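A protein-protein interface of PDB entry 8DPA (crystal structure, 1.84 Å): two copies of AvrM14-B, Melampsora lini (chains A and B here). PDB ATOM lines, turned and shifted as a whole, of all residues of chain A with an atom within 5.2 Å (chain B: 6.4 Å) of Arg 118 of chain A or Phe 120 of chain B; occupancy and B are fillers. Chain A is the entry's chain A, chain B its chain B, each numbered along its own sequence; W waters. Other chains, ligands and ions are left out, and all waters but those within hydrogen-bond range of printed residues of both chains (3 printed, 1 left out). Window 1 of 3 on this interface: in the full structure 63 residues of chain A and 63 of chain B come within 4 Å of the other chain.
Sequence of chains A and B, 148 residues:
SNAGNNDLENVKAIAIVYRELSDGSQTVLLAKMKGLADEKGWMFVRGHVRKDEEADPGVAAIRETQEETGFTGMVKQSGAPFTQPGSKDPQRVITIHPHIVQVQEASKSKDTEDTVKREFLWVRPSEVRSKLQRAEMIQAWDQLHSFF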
ATOM      1  N   LEU A  29      -1.584   9.458  26.123  1.00  0.00           N
ATOM      2  CA  LEU A  29      -1.677   8.007  26.140  1.00  0.00           C
ATOM      3  C   LEU A  29      -0.416   7.386  26.725  1.00  0.00           C
ATOM      4  O   LEU A  29       0.698   7.703  26.291  1.00  0.00           O
ATOM      5  CB  LEU A  29      -1.894   7.492  24.721  1.00  0.00           C
ATOM      6  CG  LEU A  29      -2.080   5.989  24.541  1.00  0.00           C
ATOM      7  CD1 LEU A  29      -3.424   5.514  25.093  1.00  0.00           C
ATOM      8  CD2 LEU A  29      -1.946   5.643  23.070  1.00  0.00           C
ATOM      9  N   LEU A  30      -0.590   6.491  27.689  1.00  0.00           N
ATOM     10  CA  LEU A  30       0.506   5.690  28.223  1.00  0.00           C
ATOM     11  C   LEU A  30       0.200   4.216  28.012  1.00  0.00           C
ATOM     12  O   LEU A  30      -0.965   3.818  27.835  1.00  0.00           O
ATOM     13  CB  LEU A  30       0.736   5.975  29.714  1.00  0.00           C
ATOM     14  CG  LEU A  30       1.067   7.427  30.066  1.00  0.00           C
ATOM     15  CD1 LEU A  30       1.085   7.621  31.591  1.00  0.00           C
ATOM     16  CD2 LEU A  30       2.414   7.840  29.473  1.00  0.00           C
ATOM     17  N   ALA A  31       1.257   3.405  28.044  1.00  0.00           N
ATOM     18  CA  ALA A  31       1.133   1.981  27.773  1.00  0.00           C
ATOM     19  C   ALA A  31       2.124   1.205  28.623  1.00  0.00           C
ATOM     20  O   ALA A  31       3.178   1.723  29.014  1.00  0.00           O
ATOM     21  CB  ALA A  31       1.362   1.657  26.288  1.00  0.00           C
ATOM     22  N   LYS A  32       1.797  -0.055  28.882  1.00  0.00           N
ATOM     23  CA  LYS A  32       2.769  -0.936  29.507  1.00  0.00           C
ATOM     24  C   LYS A  32       2.485  -2.357  29.066  1.00  0.00           C
ATOM     25  O   LYS A  32       1.339  -2.718  28.780  1.00  0.00           O
ATOM     26  CB  LYS A  32       2.754  -0.851  31.037  1.00  0.00           C
ATOM     27  CG  LYS A  32       1.547  -1.463  31.676  1.00  0.00           C
ATOM     28  CD  LYS A  32       1.501  -1.250  33.181  1.00  0.00           C
ATOM     29  CE  LYS A  32       0.485  -2.228  33.781  1.00  0.00           C
ATOM     30  NZ  LYS A  32       0.126  -1.983  35.210  1.00  0.00           N
ATOM     31  N   TRP A  42       4.877   3.197  33.433  1.00  0.00           N
ATOM     32  CA  TRP A  42       4.227   3.284  32.130  1.00  0.00           C
ATOM     33  C   TRP A  42       5.175   3.901  31.107  1.00  0.00           C
ATOM     34  O   TRP A  42       6.202   4.482  31.449  1.00  0.00           O
ATOM     35  CB  TRP A  42       2.942   4.114  32.229  1.00  0.00           C
ATOM     36  CG  TRP A  42       1.931   3.489  33.112  1.00  0.00           C
ATOM     37  CD1 TRP A  42       1.918   3.464  34.477  1.00  0.00           C
ATOM     38  CD2 TRP A  42       0.773   2.772  32.683  1.00  0.00           C
ATOM     39  NE1 TRP A  42       0.807   2.775  34.923  1.00  0.00           N
ATOM     40  CE2 TRP A  42       0.094   2.339  33.837  1.00  0.00           C
ATOM     41  CE3 TRP A  42       0.246   2.450  31.427  1.00  0.00           C
ATOM     42  CZ2 TRP A  42      -1.091   1.598  33.773  1.00  0.00           C
ATOM     43  CZ3 TRP A  42      -0.929   1.719  31.364  1.00  0.00           C
ATOM     44  CH2 TRP A  42      -1.584   1.297  32.533  1.00  0.00           C
ATOM     45  N   GLU A  68       1.360   0.430  17.019  1.00  0.00           N
ATOM     46  CA  GLU A  68       1.128   0.078  18.417  1.00  0.00           C
ATOM     47  C   GLU A  68      -0.286   0.381  18.883  1.00  0.00           C
ATOM     48  O   GLU A  68      -0.833  -0.363  19.710  1.00  0.00           O
ATOM     49  CB  GLU A  68       2.136   0.808  19.307  1.00  0.00           C
ATOM     50  CG  GLU A  68       3.583   0.614  18.907  1.00  0.00           C
ATOM     51  CD  GLU A  68       4.494   0.443  20.112  1.00  0.00           C
ATOM     52  OE1 GLU A  68       4.056   0.833  21.228  1.00  0.00           O
ATOM     53  OE2 GLU A  68       5.660   0.021  19.944  1.00  0.00           O
ATOM     54  N   THR A  69      -0.899   1.452  18.379  1.00  0.00           N
ATOM     55  CA  THR A  69      -2.178   1.898  18.912  1.00  0.00           C
ATOM     56  C   THR A  69      -3.327   1.833  17.921  1.00  0.00           C
ATOM     57  O   THR A  69      -4.481   1.849  18.352  1.00  0.00           O
ATOM     58  CB  THR A  69      -2.074   3.345  19.417  1.00  0.00           C
ATOM     59  OG1 THR A  69      -2.096   4.232  18.292  1.00  0.00           O
ATOM     60  CG2 THR A  69      -0.780   3.562  20.214  1.00  0.00           C
ATOM     61  N   GLU A 113     -14.668  13.333  33.078  1.00  0.00           N
ATOM     62  CA  GLU A 113     -13.676  12.447  33.690  1.00  0.00           C
ATOM     63  C   GLU A 113     -13.737  11.030  33.144  1.00  0.00           C
ATOM     64  O   GLU A 113     -12.895  10.208  33.522  1.00  0.00           O
ATOM     65  CB  GLU A 113     -13.778  12.443  35.223  1.00  0.00           C
ATOM     66  CG  GLU A 113     -12.422  12.041  35.918  1.00  0.00           C
ATOM     67  CD  GLU A 113     -11.288  13.085  35.822  1.00  0.00           C
ATOM     68  OE1 GLU A 113     -11.306  13.946  34.916  1.00  0.00           O
ATOM     69  OE2 GLU A 113     -10.334  13.009  36.630  1.00  0.00           O
ATOM     70  N   ASP A 114     -14.676  10.748  32.235  1.00  0.00           N
ATOM     71  CA  ASP A 114     -14.659   9.510  31.462  1.00  0.00           C
ATOM     72  C   ASP A 114     -13.443   9.399  30.547  1.00  0.00           C
ATOM     73  O   ASP A 114     -13.143   8.305  30.062  1.00  0.00           O
ATOM     74  CB  ASP A 114     -15.917   9.436  30.604  1.00  0.00           C
ATOM     75  CG  ASP A 114     -16.933   8.505  31.159  1.00  0.00           C
ATOM     76  OD1 ASP A 114     -17.021   8.400  32.401  1.00  0.00           O
ATOM     77  OD2 ASP A 114     -17.628   7.859  30.350  1.00  0.00           O
ATOM     78  N   VAL A 116     -10.233   9.837  31.152  1.00  0.00           N
ATOM     79  CA  VAL A 116      -8.964   9.466  31.778  1.00  0.00           C
ATOM     80  C   VAL A 116      -9.216   8.413  32.846  1.00  0.00           C
ATOM     81  O   VAL A 116     -10.360   8.101  33.199  1.00  0.00           O
ATOM     82  CB  VAL A 116      -8.237  10.665  32.418  1.00  0.00           C
ATOM     83  CG1 VAL A 116      -7.802  11.656  31.355  1.00  0.00           C
ATOM     84  CG2 VAL A 116      -9.171  11.338  33.459  1.00  0.00           C
ATOM     85  N   LYS A 117      -8.111   7.878  33.369  1.00  0.00           N
ATOM     86  CA  LYS A 117      -8.098   6.995  34.529  1.00  0.00           C
ATOM     87  C   LYS A 117      -8.787   5.657  34.277  1.00  0.00           C
ATOM     88  O   LYS A 117      -9.193   4.986  35.230  1.00  0.00           O
ATOM     89  CB  LYS A 117      -8.719   7.695  35.742  1.00  0.00           C
ATOM     90  CG  LYS A 117      -7.756   8.681  36.409  1.00  0.00           C
ATOM     91  CD  LYS A 117      -8.459   9.457  37.520  1.00  0.00           C
ATOM     92  CE  LYS A 117      -7.519  10.456  38.170  1.00  0.00           C
ATOM     93  NZ  LYS A 117      -7.246  11.622  37.267  1.00  0.00           N
ATOM     94  N   ARG A 118      -8.930   5.243  33.022  1.00  0.00           N
ATOM     95  CA  ARG A 118      -9.414   3.907  32.697  1.00  0.00           C
ATOM     96  C   ARG A 118      -8.316   3.162  31.964  1.00  0.00           C
ATOM     97  O   ARG A 118      -7.805   3.639  30.950  1.00  0.00           O
ATOM     98  CB  ARG A 118     -10.674   3.930  31.836  1.00  0.00           C
ATOM     99  CG  ARG A 118     -11.821   4.604  32.550  1.00  0.00           C
ATOM    100  CD  ARG A 118     -13.140   4.565  31.820  1.00  0.00           C
ATOM    101  NE  ARG A 118     -14.273   4.883  32.692  1.00  0.00           N
ATOM    102  CZ  ARG A 118     -14.286   5.834  33.625  1.00  0.00           C
ATOM    103  NH1 ARG A 118     -13.263   6.673  33.798  1.00  0.00           N
ATOM    104  NH2 ARG A 118     -15.359   5.973  34.388  1.00  0.00           N
ATOM    105  N   GLU A 119      -7.973   1.996  32.480  1.00  0.00           N
ATOM    106  CA  GLU A 119      -6.978   1.122  31.895  1.00  0.00           C
ATOM    107  C   GLU A 119      -7.666   0.211  30.877  1.00  0.00           C
ATOM    108  O   GLU A 119      -8.788  -0.259  31.113  1.00  0.00           O
ATOM    109  CB  GLU A 119      -6.342   0.342  33.040  1.00  0.00           C
ATOM    110  CG  GLU A 119      -5.038  -0.280  32.814  1.00  0.00           C
ATOM    111  CD  GLU A 119      -4.444  -0.711  34.142  1.00  0.00           C
ATOM    112  OE1 GLU A 119      -4.752  -0.061  35.165  1.00  0.00           O
ATOM    113  OE2 GLU A 119      -3.661  -1.665  34.170  1.00  0.00           O
ATOM    114  N   PHE A 120      -7.014  -0.005  29.726  1.00  0.00           N
ATOM    115  CA  PHE A 120      -7.597  -0.736  28.597  1.00  0.00           C
ATOM    116  C   PHE A 120      -6.708  -1.893  28.161  1.00  0.00           C
ATOM    117  O   PHE A 120      -5.474  -1.795  28.191  1.00  0.00           O
ATOM    118  CB  PHE A 120      -7.805   0.171  27.378  1.00  0.00           C
ATOM    119  CG  PHE A 120      -8.817   1.241  27.592  1.00  0.00           C
ATOM    120  CD1 PHE A 120     -10.169   0.937  27.627  1.00  0.00           C
ATOM    121  CD2 PHE A 120      -8.421   2.553  27.771  1.00  0.00           C
ATOM    122  CE1 PHE A 120     -11.125   1.945  27.834  1.00  0.00           C
ATOM    123  CE2 PHE A 120      -9.357   3.555  27.972  1.00  0.00           C
ATOM    124  CZ  PHE A 120     -10.720   3.245  28.010  1.00  0.00           C
ATOM    125  N   LEU A 121      -7.355  -2.965  27.692  1.00  0.00           N
ATOM    126  CA  LEU A 121      -6.682  -4.180  27.244  1.00  0.00           C
ATOM    127  C   LEU A 121      -7.475  -4.784  26.088  1.00  0.00           C
ATOM    128  O   LEU A 121      -8.697  -4.938  26.197  1.00  0.00           O
ATOM    129  CB  LEU A 121      -6.584  -5.194  28.397  1.00  0.00           C
ATOM    130  CG  LEU A 121      -5.825  -6.497  28.166  1.00  0.00           C
ATOM    131  CD1 LEU A 121      -4.357  -6.229  27.798  1.00  0.00           C
ATOM    132  CD2 LEU A 121      -5.942  -7.405  29.371  1.00  0.00           C
ATOM    133  N   TRP A 122      -6.798  -5.118  24.983  1.00  0.00           N
ATOM    134  CA  TRP A 122      -7.441  -5.825  23.878  1.00  0.00           C
ATOM    135  C   TRP A 122      -7.247  -7.323  24.059  1.00  0.00           C
ATOM    136  O   TRP A 122      -6.120  -7.774  24.281  1.00  0.00           O
ATOM    137  CB  TRP A 122      -6.871  -5.414  22.519  1.00  0.00           C
ATOM    138  CG  TRP A 122      -7.142  -3.997  22.085  1.00  0.00           C
ATOM    139  CD1 TRP A 122      -6.357  -2.898  22.301  1.00  0.00           C
ATOM    140  CD2 TRP A 122      -8.305  -3.531  21.393  1.00  0.00           C
ATOM    141  NE1 TRP A 122      -6.948  -1.780  21.754  1.00  0.00           N
ATOM    142  CE2 TRP A 122      -8.153  -2.143  21.201  1.00  0.00           C
ATOM    143  CE3 TRP A 122      -9.474  -4.159  20.923  1.00  0.00           C
ATOM    144  CZ2 TRP A 122      -9.116  -1.369  20.544  1.00  0.00           C
ATOM    145  CZ3 TRP A 122     -10.431  -3.390  20.265  1.00  0.00           C
ATOM    146  CH2 TRP A 122     -10.249  -2.007  20.089  1.00  0.00           C
ATOM    147  N   ARG B  19     -12.263  -4.664  17.088  1.00  0.00           N
ATOM    148  CA  ARG B  19     -11.735  -4.309  15.780  1.00  0.00           C
ATOM    149  C   ARG B  19     -11.313  -5.567  15.050  1.00  0.00           C
ATOM    150  O   ARG B  19     -11.060  -6.608  15.666  1.00  0.00           O
ATOM    151  CB  ARG B  19     -10.607  -3.287  15.898  1.00  0.00           C
ATOM    152  CG  ARG B  19      -9.427  -3.724  16.650  1.00  0.00           C
ATOM    153  CD  ARG B  19      -8.476  -2.529  16.711  1.00  0.00           C
ATOM    154  NE  ARG B  19      -7.339  -2.800  17.566  1.00  0.00           N
ATOM    155  CZ  ARG B  19      -6.488  -1.876  17.997  1.00  0.00           C
ATOM    156  NH1 ARG B  19      -6.626  -0.597  17.673  1.00  0.00           N
ATOM    157  NH2 ARG B  19      -5.503  -2.239  18.806  1.00  0.00           N
ATOM    158  N   LEU B  29     -12.152  -4.924  23.172  1.00  0.00           N
ATOM    159  CA  LEU B  29     -11.581  -3.988  24.134  1.00  0.00           C
ATOM    160  C   LEU B  29     -12.223  -4.135  25.510  1.00  0.00           C
ATOM    161  O   LEU B  29     -13.444  -4.049  25.643  1.00  0.00           O
ATOM    162  CB  LEU B  29     -11.761  -2.556  23.635  1.00  0.00           C
ATOM    163  CG  LEU B  29     -11.101  -1.503  24.514  1.00  0.00           C
ATOM    164  CD1 LEU B  29      -9.590  -1.679  24.487  1.00  0.00           C
ATOM    165  CD2 LEU B  29     -11.467  -0.126  24.023  1.00  0.00           C
ATOM    166  N   ALA B  31     -11.980  -2.814  29.747  1.00  0.00           N
ATOM    167  CA  ALA B  31     -11.549  -1.668  30.530  1.00  0.00           C
ATOM    168  C   ALA B  31     -11.697  -1.967  32.010  1.00  0.00           C
ATOM    169  O   ALA B  31     -12.522  -2.791  32.420  1.00  0.00           O
ATOM    170  CB  ALA B  31     -12.359  -0.410  30.176  1.00  0.00           C
ATOM    171  N   LYS B  32     -10.895  -1.276  32.819  1.00  0.00           N
ATOM    172  CA  LYS B  32     -11.258  -1.119  34.219  1.00  0.00           C
ATOM    173  C   LYS B  32     -10.797   0.237  34.718  1.00  0.00           C
ATOM    174  O   LYS B  32      -9.830   0.827  34.207  1.00  0.00           O
ATOM    175  CB  LYS B  32     -10.658  -2.148  35.170  1.00  0.00           C
ATOM    176  CG  LYS B  32      -9.149  -2.146  35.242  1.00  0.00           C
ATOM    177  CD  LYS B  32      -8.711  -3.237  36.204  1.00  0.00           C
ATOM    178  CE  LYS B  32      -8.475  -4.547  35.526  1.00  0.00           C
ATOM    179  NZ  LYS B  32      -8.584  -5.721  36.443  1.00  0.00           N
ATOM    180  N   MET B  33     -11.475   0.698  35.763  1.00  0.00           N
ATOM    181  CA  MET B  33     -11.033   1.890  36.470  1.00  0.00           C
ATOM    182  C   MET B  33      -9.686   1.631  37.133  1.00  0.00           C
ATOM    183  O   MET B  33      -9.525   0.653  37.867  1.00  0.00           O
ATOM    184  CB  MET B  33     -12.074   2.303  37.507  1.00  0.00           C
ATOM    185  CG  MET B  33     -13.243   3.032  36.898  1.00  0.00           C
ATOM    186  SD  MET B  33     -12.805   4.745  36.524  1.00  0.00           S
ATOM    187  CE  MET B  33     -11.653   5.132  37.847  1.00  0.00           C
ATOM    188  N   LYS B  34      -8.716   2.505  36.871  1.00  0.00           N
ATOM    189  CA  LYS B  34      -7.363   2.284  37.370  1.00  0.00           C
ATOM    190  C   LYS B  34      -7.333   2.379  38.893  1.00  0.00           C
ATOM    191  O   LYS B  34      -7.727   3.400  39.470  1.00  0.00           O
ATOM    192  CB  LYS B  34      -6.403   3.294  36.739  1.00  0.00           C
ATOM    193  CG  LYS B  34      -5.145   3.576  37.545  1.00  0.00           C
ATOM    194  CD  LYS B  34      -3.906   3.548  36.651  1.00  0.00           C
ATOM    195  CE  LYS B  34      -2.711   4.239  37.308  1.00  0.00           C
ATOM    196  NZ  LYS B  34      -1.955   3.373  38.267  1.00  0.00           N
ATOM    197  N   MET B  43     -14.471  -4.713  32.325  1.00  0.00           N
ATOM    198  CA  MET B  43     -15.795  -4.333  31.886  1.00  0.00           C
ATOM    199  C   MET B  43     -15.739  -3.834  30.448  1.00  0.00           C
ATOM    200  O   MET B  43     -14.665  -3.626  29.862  1.00  0.00           O
ATOM    201  CB  MET B  43     -16.387  -3.289  32.847  1.00  0.00           C
ATOM    202  CG  MET B  43     -15.769  -1.911  32.785  1.00  0.00           C
ATOM    203  SD  MET B  43     -16.505  -0.840  34.042  1.00  0.00           S
ATOM    204  CE  MET B  43     -17.423   0.308  33.022  1.00  0.00           C
ATOM    205  N   ARG B  46     -19.301   1.779  29.137  1.00  0.00           N
ATOM    206  CA  ARG B  46     -20.652   2.023  29.646  1.00  0.00           C
ATOM    207  C   ARG B  46     -20.833   3.510  29.909  1.00  0.00           C
ATOM    208  O   ARG B  46     -19.882   4.199  30.274  1.00  0.00           O
ATOM    209  CB  ARG B  46     -20.918   1.250  30.945  1.00  0.00           C
ATOM    210  CG  ARG B  46     -22.311   1.480  31.537  1.00  0.00           C
ATOM    211  CD  ARG B  46     -22.537   0.663  32.803  1.00  0.00           C
ATOM    212  NE  ARG B  46     -21.926   1.350  33.936  1.00  0.00           N
ATOM    213  CZ  ARG B  46     -21.438   0.753  35.015  1.00  0.00           C
ATOM    214  NH1 ARG B  46     -21.615  -0.542  35.233  1.00  0.00           N
ATOM    215  NH2 ARG B  46     -20.769   1.479  35.909  1.00  0.00           N
ATOM    216  N   GLU B  68     -14.192   7.523  25.920  1.00  0.00           N
ATOM    217  CA  GLU B  68     -13.309   6.721  26.765  1.00  0.00           C
ATOM    218  C   GLU B  68     -12.030   6.310  26.044  1.00  0.00           C
ATOM    219  O   GLU B  68     -10.948   6.320  26.643  1.00  0.00           O
ATOM    220  CB  GLU B  68     -14.051   5.481  27.269  1.00  0.00           C
ATOM    221  CG  GLU B  68     -15.200   5.813  28.207  1.00  0.00           C
ATOM    222  CD  GLU B  68     -15.674   4.611  29.015  1.00  0.00           C
ATOM    223  OE1 GLU B  68     -15.026   3.548  28.973  1.00  0.00           O
ATOM    224  OE2 GLU B  68     -16.680   4.742  29.729  1.00  0.00           O
ATOM    225  N   VAL B 116      -2.733  -4.882  21.091  1.00  0.00           N
ATOM    226  CA  VAL B 116      -3.042  -6.225  21.574  1.00  0.00           C
ATOM    227  C   VAL B 116      -2.111  -6.620  22.720  1.00  0.00           C
ATOM    228  O   VAL B 116      -2.546  -7.183  23.727  1.00  0.00           O
ATOM    229  CB  VAL B 116      -2.970  -7.261  20.428  1.00  0.00           C
ATOM    230  CG1 VAL B 116      -2.596  -8.644  20.959  1.00  0.00           C
ATOM    231  CG2 VAL B 116      -4.294  -7.321  19.685  1.00  0.00           C
ATOM    232  N   LYS B 117      -0.827  -6.301  22.565  1.00  0.00           N
ATOM    233  CA  LYS B 117       0.184  -6.741  23.522  1.00  0.00           C
ATOM    234  C   LYS B 117       0.141  -5.947  24.827  1.00  0.00           C
ATOM    235  O   LYS B 117       0.410  -6.501  25.902  1.00  0.00           O
ATOM    236  CB  LYS B 117       1.569  -6.625  22.885  1.00  0.00           C
ATOM    237  CG  LYS B 117       1.716  -7.431  21.614  1.00  0.00           C
ATOM    238  CD  LYS B 117       3.141  -7.387  21.117  1.00  0.00           C
ATOM    239  CE  LYS B 117       4.076  -7.852  22.212  1.00  0.00           C
ATOM    240  NZ  LYS B 117       3.918  -9.312  22.452  1.00  0.00           N
ATOM    241  N   ARG B 118      -0.195  -4.666  24.760  1.00  0.00           N
ATOM    242  CA  ARG B 118      -0.021  -3.767  25.886  1.00  0.00           C
ATOM    243  C   ARG B 118      -1.354  -3.342  26.476  1.00  0.00           C
ATOM    244  O   ARG B 118      -2.409  -3.450  25.848  1.00  0.00           O
ATOM    245  CB  ARG B 118       0.790  -2.532  25.481  1.00  0.00           C
ATOM    246  CG  ARG B 118       1.891  -2.819  24.425  1.00  0.00           C
ATOM    247  CD  ARG B 118       2.590  -1.527  24.043  1.00  0.00           C
ATOM    248  NE  ARG B 118       3.865  -1.735  23.364  1.00  0.00           N
ATOM    249  CZ  ARG B 118       4.030  -2.369  22.211  1.00  0.00           C
ATOM    250  NH1 ARG B 118       3.000  -2.809  21.507  1.00  0.00           N
ATOM    251  NH2 ARG B 118       5.260  -2.531  21.732  1.00  0.00           N
ATOM    252  N   GLU B 119      -1.272  -2.879  27.714  1.00  0.00           N
ATOM    253  CA  GLU B 119      -2.365  -2.211  28.390  1.00  0.00           C
ATOM    254  C   GLU B 119      -2.187  -0.715  28.165  1.00  0.00           C
ATOM    255  O   GLU B 119      -1.051  -0.226  28.121  1.00  0.00           O
ATOM    256  CB  GLU B 119      -2.309  -2.533  29.880  1.00  0.00           C
ATOM    257  CG  GLU B 119      -3.018  -3.812  30.250  1.00  0.00           C
ATOM    258  CD  GLU B 119      -3.272  -3.925  31.733  1.00  0.00           C
ATOM    259  OE1 GLU B 119      -3.647  -2.906  32.334  1.00  0.00           O
ATOM    260  OE2 GLU B 119      -3.029  -5.012  32.308  1.00  0.00           O
ATOM    261  N   PHE B 120      -3.295   0.014  28.013  1.00  0.00           N
ATOM    262  CA  PHE B 120      -3.221   1.442  27.737  1.00  0.00           C
ATOM    263  C   PHE B 120      -3.975   2.242  28.790  1.00  0.00           C
ATOM    264  O   PHE B 120      -4.891   1.734  29.454  1.00  0.00           O
ATOM    265  CB  PHE B 120      -3.796   1.804  26.362  1.00  0.00           C
ATOM    266  CG  PHE B 120      -3.133   1.099  25.228  1.00  0.00           C
ATOM    267  CD1 PHE B 120      -3.486  -0.206  24.901  1.00  0.00           C
ATOM    268  CD2 PHE B 120      -2.061   1.689  24.568  1.00  0.00           C
ATOM    269  CE1 PHE B 120      -2.852  -0.878  23.852  1.00  0.00           C
ATOM    270  CE2 PHE B 120      -1.406   1.023  23.533  1.00  0.00           C
ATOM    271  CZ  PHE B 120      -1.804  -0.262  23.172  1.00  0.00           C
ATOM    272  N   LEU B 121      -3.615   3.527  28.884  1.00  0.00           N
ATOM    273  CA  LEU B 121      -4.219   4.429  29.851  1.00  0.00           C
ATOM    274  C   LEU B 121      -4.124   5.866  29.360  1.00  0.00           C
ATOM    275  O   LEU B 121      -3.070   6.291  28.872  1.00  0.00           O
ATOM    276  CB  LEU B 121      -3.554   4.270  31.230  1.00  0.00           C
ATOM    277  CG  LEU B 121      -3.981   5.267  32.307  1.00  0.00           C
ATOM    278  CD1 LEU B 121      -5.318   4.821  32.916  1.00  0.00           C
ATOM    279  CD2 LEU B 121      -2.927   5.261  33.402  1.00  0.00           C
ATOM    280  N   TRP B 122      -5.226   6.609  29.465  1.00  0.00           N
ATOM    281  CA  TRP B 122      -5.215   8.032  29.150  1.00  0.00           C
ATOM    282  C   TRP B 122      -5.048   8.807  30.445  1.00  0.00           C
ATOM    283  O   TRP B 122      -5.688   8.482  31.451  1.00  0.00           O
ATOM    284  CB  TRP B 122      -6.501   8.484  28.449  1.00  0.00           C
ATOM    285  CG  TRP B 122      -6.685   7.981  27.047  1.00  0.00           C
ATOM    286  CD1 TRP B 122      -7.522   6.973  26.640  1.00  0.00           C
ATOM    287  CD2 TRP B 122      -6.041   8.474  25.855  1.00  0.00           C
ATOM    288  NE1 TRP B 122      -7.432   6.805  25.274  1.00  0.00           N
ATOM    289  CE2 TRP B 122      -6.532   7.711  24.768  1.00  0.00           C
ATOM    290  CE3 TRP B 122      -5.099   9.481  25.603  1.00  0.00           C
ATOM    291  CZ2 TRP B 122      -6.122   7.934  23.446  1.00  0.00           C
ATOM    292  CZ3 TRP B 122      -4.683   9.698  24.277  1.00  0.00           C
ATOM    293  CH2 TRP B 122      -5.190   8.924  23.222  1.00  0.00           C
HETATM  294  O   HOH W   1     -10.579   6.778  29.266  1.00  0.00           O
HETATM  295  O   HOH W   2       0.296  -2.483  21.360  1.00  0.00           O
HETATM  296  O   HOH W   3      -8.101   6.065  30.295  1.00  0.00           O
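N of Leu 30 of chain A is in hydrogen-bond range of O of Leu 121 of chain B, 2.8 Å away.
O of Lys 32 of chain A is in hydrogen-bond range of N of Glu 119 of chain B, 2.8 Å away.
NH2 of Arg 118 of chain B is in salt-bridge range of OE2 of Glu 68 of chain A (3.1 Å).
The backbone carbonyl oxygen of Thr 69 of chain A lies within hydrogen-bond range of the guanidinium group of Arg 19 of chain B.
O of Lys 117 of chain A is in hydrogen-bond range of N of Lys 34 of chain B, 3.0 Å away.
O of Trp 122 of chain B sits at hydrogen-bond distance from N of Lys 117 of chain A.
The side-chain sulfur (SD) of Met 33 of chain B lies within hydrogen-bond range of the guanidinium group (NH1) of Arg 118 of chain A, at 3.4 Å.
NE of Arg 118 of chain A lies within salt-bridge range of OE2 of Glu 68 of chain B (3.8 Å).
The backbone carbonyl oxygen of Lys 32 of chain B lies within hydrogen-bond range of the backbone NH of Glu 119 of chain A, 2.8 Å away.
N of Phe 120 of chain A lies within hydrogen-bond range of O of Phe 120 of chain B, at 2.8 Å.
The side-chain carboxylate (OD2) of Asp 114 of chain A lies close to the side-chain carboxylate (OE2) of Glu 68 of chain B (3.3 Å).
OE1 of Glu 119 of chain B lies close to OE2 of Glu 119 of chain A (2.2 Å).
The indole nitrogen of Trp 122 of chain A lies close to the guanidinium group of Arg 19 of chain B.
The side-chain amino group of Lys 32 of chain A lies within salt-bridge range of the side-chain carboxylate of Glu 119 of chain A, 3.9 Å away.
OE2 of Glu 113 of chain A is in salt-bridge range of NZ of Lys 117 of chain A, at 3.4 Å.
O of Val 116 of chain A lies within hydrogen-bond range of NH1 of Arg 118 of chain A, 3.3 Å away.
CB of Arg 118 of chain B touches O of Lys 32 of chain A, 3.3 Å away.
Lys 32 of chain B touches Arg 118 of chain A.
O of Glu 119 of chain A touches CA of Ala 31 of chain B (3.2 Å).
Glu 119 of chain A touches Phe 120 of chain B (CA to O, 3.3 Å).
Phe 120 of chain A touches Leu 29 of chain B (CB to CD1, 3.9 Å).
Leu 121 of chain A touches Leu 29 of chain B.
Arg 118 of chain A touches five residues of chain B.
Printed residues of chain A within 4 Å of Phe 120 of chain B: Leu 29, Leu 30, Ala 31, Glu 68, Arg 118, Glu 119 and Phe 120.
Of the printed residues of chain B, Leu 30 of chain A touches Phe 120 (3.3 Å) and Leu 121 (2.8 Å).
Of the printed residues of chain A, Arg 118 of chain B touches Lys 32 (3.3 Å), Glu 68 (3.1 Å) and Leu 121 (3.9 Å).
The nearest residue of chain A that does not touch Phe 120 of chain B is Trp 42 of chain A (4.02 Å).
The nearest printed residue of chain A that does not touch Arg 118 of chain B is Ala 31 of chain A (4.1 Å).
Of the 16 printed residues of chain A, 15 touch a printed residue of chain B.
Hydrophobic or aromatic side chains of chain A within 4 Å of the printed part of chain B: Leu 29, Leu 30, Ala 31, Trp 42, Val 116, Phe 120, Leu 121 and Trp 122.
Hydrophobic or aromatic side chains of chain B within 4 Å of the printed part of chain A: Leu 29, Ala 31, Met 33, Phe 120, Leu 121 and Trp 122.
Leu 29 of chain A touches Phe 120 of chain B, and with the chains exchanged Phe 120 of chain A touches Leu 29 of chain B.
Ala 31 of chain A touches Phe 120 of chain B, and with the chains exchanged Phe 120 of chain A touches Ala 31 of chain B.
Positions printed for both chains: 29, 31, 32, 68, 116, 117, 118, 119, 120, 121 and 122.
Water W3 lies within hydrogen-bond range of O of Arg 118 of chain A (2.5 Å) and N of Trp 122 of chain B (3.0 Å).
Water W2 lies within hydrogen-bond range of the guanidinium group (NH1) of Arg 118 of chain B (2.7 Å) and the backbone carbonyl oxygen (O) of Glu 68 of chain A (2.9 Å).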
